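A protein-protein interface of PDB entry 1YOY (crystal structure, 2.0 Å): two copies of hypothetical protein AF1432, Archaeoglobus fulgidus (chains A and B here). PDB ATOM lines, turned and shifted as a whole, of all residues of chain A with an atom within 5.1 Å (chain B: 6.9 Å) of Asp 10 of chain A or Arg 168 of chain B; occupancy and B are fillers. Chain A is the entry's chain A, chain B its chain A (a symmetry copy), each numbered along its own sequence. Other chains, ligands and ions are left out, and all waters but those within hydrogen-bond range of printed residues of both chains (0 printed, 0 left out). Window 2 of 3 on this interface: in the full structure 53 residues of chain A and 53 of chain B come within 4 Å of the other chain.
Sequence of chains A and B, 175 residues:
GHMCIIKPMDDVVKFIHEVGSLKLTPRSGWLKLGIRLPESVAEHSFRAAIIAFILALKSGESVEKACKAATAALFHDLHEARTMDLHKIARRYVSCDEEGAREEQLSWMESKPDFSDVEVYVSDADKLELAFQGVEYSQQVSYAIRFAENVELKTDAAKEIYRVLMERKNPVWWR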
ATOM      1  N   MET A   9      21.883 -10.008 -29.456  1.00  0.00           N
ATOM      2  CA  MET A   9      21.426  -8.884 -30.322  1.00  0.00           C
ATOM      3  C   MET A   9      21.850  -7.535 -29.710  1.00  0.00           C
ATOM      4  O   MET A   9      21.841  -6.513 -30.393  1.00  0.00           O
ATOM      5  CB  MET A   9      19.914  -8.971 -30.596  1.00  0.00           C
ATOM      6  CG  MET A   9      19.432  -8.784 -32.068  1.00  0.00           C
ATOM      7  SD  MET A   9      20.323  -9.622 -33.457  1.00  0.00           S
ATOM      8  CE  MET A   9      18.988 -10.110 -34.576  1.00  0.00           C
ATOM      9  N   ASP A  10      22.280  -7.534 -28.452  1.00  0.00           N
ATOM     10  CA  ASP A  10      22.727  -6.287 -27.816  1.00  0.00           C
ATOM     11  C   ASP A  10      23.914  -5.575 -28.467  1.00  0.00           C
ATOM     12  O   ASP A  10      23.925  -4.337 -28.553  1.00  0.00           O
ATOM     13  CB  ASP A  10      23.041  -6.513 -26.347  1.00  0.00           C
ATOM     14  CG  ASP A  10      21.811  -6.896 -25.554  1.00  0.00           C
ATOM     15  OD1 ASP A  10      21.281  -5.986 -24.869  1.00  0.00           O
ATOM     16  OD2 ASP A  10      21.365  -8.079 -25.648  1.00  0.00           O
ATOM     17  N   ASP A  11      24.936  -6.342 -28.856  1.00  0.00           N
ATOM     18  CA  ASP A  11      26.120  -5.792 -29.521  1.00  0.00           C
ATOM     19  C   ASP A  11      25.817  -5.294 -30.955  1.00  0.00           C
ATOM     20  O   ASP A  11      26.466  -4.353 -31.431  1.00  0.00           O
ATOM     21  CB  ASP A  11      27.228  -6.832 -29.595  1.00  0.00           C
ATOM     22  CG  ASP A  11      27.945  -7.045 -28.251  1.00  0.00           C
ATOM     23  OD1 ASP A  11      27.867  -6.181 -27.325  1.00  0.00           O
ATOM     24  OD2 ASP A  11      28.642  -8.095 -28.143  1.00  0.00           O
ATOM     25  N   VAL A  12      24.864  -5.943 -31.619  1.00  0.00           N
ATOM     26  CA  VAL A  12      24.377  -5.538 -32.939  1.00  0.00           C
ATOM     27  C   VAL A  12      23.627  -4.173 -32.815  1.00  0.00           C
ATOM     28  O   VAL A  12      23.806  -3.277 -33.639  1.00  0.00           O
ATOM     29  CB  VAL A  12      23.411  -6.614 -33.535  1.00  0.00           C
ATOM     30  CG1 VAL A  12      22.656  -6.071 -34.729  1.00  0.00           C
ATOM     31  CG2 VAL A  12      24.158  -7.901 -33.923  1.00  0.00           C
ATOM     32  N   VAL A  13      22.808  -4.038 -31.783  1.00  0.00           N
ATOM     33  CA  VAL A  13      22.106  -2.771 -31.494  1.00  0.00           C
ATOM     34  C   VAL A  13      23.105  -1.639 -31.214  1.00  0.00           C
ATOM     35  O   VAL A  13      22.983  -0.526 -31.795  1.00  0.00           O
ATOM     36  CB  VAL A  13      21.077  -2.943 -30.331  1.00  0.00           C
ATOM     37  CG1 VAL A  13      20.578  -1.552 -29.812  1.00  0.00           C
ATOM     38  CG2 VAL A  13      19.886  -3.836 -30.787  1.00  0.00           C
ATOM     39  N   LYS A  14      24.125  -1.930 -30.385  1.00  0.00           N
ATOM     40  CA  LYS A  14      25.195  -0.954 -30.108  1.00  0.00           C
ATOM     41  C   LYS A  14      25.906  -0.555 -31.397  1.00  0.00           C
ATOM     42  O   LYS A  14      26.170   0.630 -31.598  1.00  0.00           O
ATOM     43  CB  LYS A  14      26.240  -1.510 -29.106  1.00  0.00           C
ATOM     44  CG  LYS A  14      25.943  -1.199 -27.647  1.00  0.00           C
ATOM     45  CD  LYS A  14      27.217  -1.333 -26.692  1.00  0.00           C
ATOM     46  CE  LYS A  14      26.984  -0.571 -25.375  1.00  0.00           C
ATOM     47  NZ  LYS A  14      26.397  -1.368 -24.197  1.00  0.00           N
ATOM     48  N   VAL B 135      14.897   7.061 -31.333  1.00  0.00           N
ATOM     49  CA  VAL B 135      15.567   6.834 -30.047  1.00  0.00           C
ATOM     50  C   VAL B 135      16.707   7.854 -29.795  1.00  0.00           C
ATOM     51  O   VAL B 135      16.769   8.473 -28.715  1.00  0.00           O
ATOM     52  CB  VAL B 135      16.042   5.346 -29.888  1.00  0.00           C
ATOM     53  CG1 VAL B 135      16.866   5.134 -28.604  1.00  0.00           C
ATOM     54  CG2 VAL B 135      14.831   4.391 -29.834  1.00  0.00           C
ATOM     55  N   ARG B 163      13.138  -5.046 -30.732  1.00  0.00           N
ATOM     56  CA  ARG B 163      12.880  -5.326 -29.326  1.00  0.00           C
ATOM     57  C   ARG B 163      14.011  -4.883 -28.387  1.00  0.00           C
ATOM     58  O   ARG B 163      13.768  -4.212 -27.352  1.00  0.00           O
ATOM     59  CB  ARG B 163      12.584  -6.812 -29.149  1.00  0.00           C
ATOM     60  CG  ARG B 163      12.189  -7.146 -27.736  1.00  0.00           C
ATOM     61  CD  ARG B 163      12.030  -8.650 -27.508  1.00  0.00           C
ATOM     62  NE  ARG B 163      11.731  -8.913 -26.094  1.00  0.00           N
ATOM     63  CZ  ARG B 163      11.765 -10.113 -25.501  1.00  0.00           C
ATOM     64  NH1 ARG B 163      12.097 -11.205 -26.176  1.00  0.00           N
ATOM     65  NH2 ARG B 163      11.461 -10.205 -24.204  1.00  0.00           N
ATOM     66  N   VAL B 164      15.238  -5.233 -28.762  1.00  0.00           N
ATOM     67  CA  VAL B 164      16.390  -4.907 -28.014  1.00  0.00           C
ATOM     68  C   VAL B 164      16.582  -3.379 -28.035  1.00  0.00           C
ATOM     69  O   VAL B 164      16.930  -2.794 -27.018  1.00  0.00           O
ATOM     70  CB  VAL B 164      17.673  -5.668 -28.517  1.00  0.00           C
ATOM     71  CG1 VAL B 164      18.946  -5.250 -27.737  1.00  0.00           C
ATOM     72  CG2 VAL B 164      17.481  -7.202 -28.369  1.00  0.00           C
ATOM     73  N   LEU B 165      16.374  -2.752 -29.196  1.00  0.00           N
ATOM     74  CA  LEU B 165      16.524  -1.289 -29.341  1.00  0.00           C
ATOM     75  C   LEU B 165      15.626  -0.551 -28.355  1.00  0.00           C
ATOM     76  O   LEU B 165      16.061   0.404 -27.680  1.00  0.00           O
ATOM     77  CB  LEU B 165      16.152  -0.859 -30.759  1.00  0.00           C
ATOM     78  CG  LEU B 165      15.966   0.659 -31.009  1.00  0.00           C
ATOM     79  CD1 LEU B 165      17.256   1.440 -30.888  1.00  0.00           C
ATOM     80  CD2 LEU B 165      15.189   0.991 -32.316  1.00  0.00           C
ATOM     81  N   MET B 166      14.372  -0.999 -28.298  1.00  0.00           N
ATOM     82  CA  MET B 166      13.380  -0.441 -27.406  1.00  0.00           C
ATOM     83  C   MET B 166      13.561  -0.847 -25.949  1.00  0.00           C
ATOM     84  O   MET B 166      13.171  -0.102 -25.065  1.00  0.00           O
ATOM     85  CB  MET B 166      11.958  -0.684 -27.936  1.00  0.00           C
ATOM     86  CG  MET B 166      11.771  -0.024 -29.364  1.00  0.00           C
ATOM     87  SD  MET B 166      12.108   1.774 -29.504  1.00  0.00           S
ATOM     88  CE  MET B 166      10.489   2.323 -28.963  1.00  0.00           C
ATOM     89  N   GLU B 167      14.174  -1.997 -25.684  1.00  0.00           N
ATOM     90  CA  GLU B 167      14.397  -2.383 -24.279  1.00  0.00           C
ATOM     91  C   GLU B 167      15.581  -1.631 -23.659  1.00  0.00           C
ATOM     92  O   GLU B 167      15.536  -1.263 -22.485  1.00  0.00           O
ATOM     93  CB  GLU B 167      14.478  -3.912 -24.110  1.00  0.00           C
ATOM     94  CG  GLU B 167      15.842  -4.497 -24.013  1.00  0.00           C
ATOM     95  CD  GLU B 167      15.821  -6.027 -24.135  1.00  0.00           C
ATOM     96  OE1 GLU B 167      16.914  -6.590 -24.403  1.00  0.00           O
ATOM     97  OE2 GLU B 167      14.731  -6.648 -23.990  1.00  0.00           O
ATOM     98  N   ARG B 168      16.619  -1.355 -24.455  1.00  0.00           N
ATOM     99  CA  ARG B 168      17.749  -0.548 -23.983  1.00  0.00           C
ATOM    100  C   ARG B 168      17.405   0.956 -23.998  1.00  0.00           C
ATOM    101  O   ARG B 168      17.631   1.644 -23.003  1.00  0.00           O
ATOM    102  CB  ARG B 168      19.033  -0.843 -24.786  1.00  0.00           C
ATOM    103  CG  ARG B 168      19.206  -2.307 -25.227  1.00  0.00           C
ATOM    104  CD  ARG B 168      19.935  -3.226 -24.226  1.00  0.00           C
ATOM    105  NE  ARG B 168      19.177  -3.569 -23.005  1.00  0.00           N
ATOM    106  CZ  ARG B 168      19.530  -4.516 -22.122  1.00  0.00           C
ATOM    107  NH1 ARG B 168      18.779  -4.739 -21.035  1.00  0.00           N
ATOM    108  NH2 ARG B 168      20.631  -5.248 -22.316  1.00  0.00           N
ATOM    109  N   LYS B 169      16.832   1.445 -25.104  1.00  0.00           N
ATOM    110  CA  LYS B 169      16.720   2.901 -25.390  1.00  0.00           C
ATOM    111  C   LYS B 169      18.009   3.673 -24.977  1.00  0.00           C
ATOM    112  O   LYS B 169      17.981   4.706 -24.305  1.00  0.00           O
ATOM    113  CB  LYS B 169      15.448   3.521 -24.784  1.00  0.00           C
ATOM    114  CG  LYS B 169      14.176   3.118 -25.490  1.00  0.00           C
ATOM    115  CD  LYS B 169      13.002   3.978 -25.064  1.00  0.00           C
ATOM    116  CE  LYS B 169      11.687   3.349 -25.503  1.00  0.00           C
ATOM    117  NZ  LYS B 169      11.391   2.116 -24.697  1.00  0.00           N
ATOM    118  N   ASN B 170      19.154   3.132 -25.388  1.00  0.00           N
ATOM    119  CA  ASN B 170      20.423   3.708 -25.004  1.00  0.00           C
ATOM    120  C   ASN B 170      21.318   3.938 -26.216  1.00  0.00           C
ATOM    121  O   ASN B 170      22.022   3.028 -26.648  1.00  0.00           O
ATOM    122  CB  ASN B 170      21.135   2.806 -24.004  1.00  0.00           C
ATOM    123  CG  ASN B 170      22.336   3.462 -23.429  1.00  0.00           C
ATOM    124  OD1 ASN B 170      22.604   4.660 -23.716  1.00  0.00           O
ATOM    125  ND2 ASN B 170      23.098   2.703 -22.623  1.00  0.00           N
ATOM    126  N   PRO B 171      21.317   5.167 -26.749  1.00  0.00           N
ATOM    127  CA  PRO B 171      22.146   5.456 -27.934  1.00  0.00           C
ATOM    128  C   PRO B 171      23.638   5.686 -27.635  1.00  0.00           C
ATOM    129  O   PRO B 171      24.430   5.925 -28.553  1.00  0.00           O
ATOM    130  CB  PRO B 171      21.473   6.698 -28.527  1.00  0.00           C
ATOM    131  CG  PRO B 171      20.877   7.395 -27.337  1.00  0.00           C
ATOM    132  CD  PRO B 171      20.508   6.323 -26.330  1.00  0.00           C
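The side-chain carboxylate (OD1) of Asp 10 of chain A lies within salt-bridge range of the guanidinium group (NH2) of Arg 168 of chain B, 2.7 Å away.
Val 164 of chain B touches Met 9 of chain A (CG2 to CB, 3.7 Å). Asp 10 of chain A touches Val 164 of chain B. Val 164 of chain B touches Val 13 of chain A.
Asp 10 of chain A touches just these residues of chain B: Val 164 (3.8 Å) and Arg 168 (2.7 Å). Arg 168 of chain B touches just one residue of chain A: Asp 10 (2.7 Å). Of the printed residues of chain B, Met 9 of chain A touches Val 164 (3.7 Å). Printed residues of chain B within 4 Å of Val 13 of chain A: Val 164 (3.5 Å). Asp 11 of chain A touches none of the printed residues of chain B. Lys 14 of chain A touches none of the printed residues of chain B. The nearest residue of chain B that does not touch Asp 10 of chain A is Glu 167 of chain B (4.4 Å).
Of the 10 printed residues of chain B, 2 touch a printed residue of chain A. Among the printed residues, 4 pairs touch across the chains.
No position is printed for both chains. Of the 4 pairs that touch across the chains among the printed residues, none has its exchanged pair printed and touching as well.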
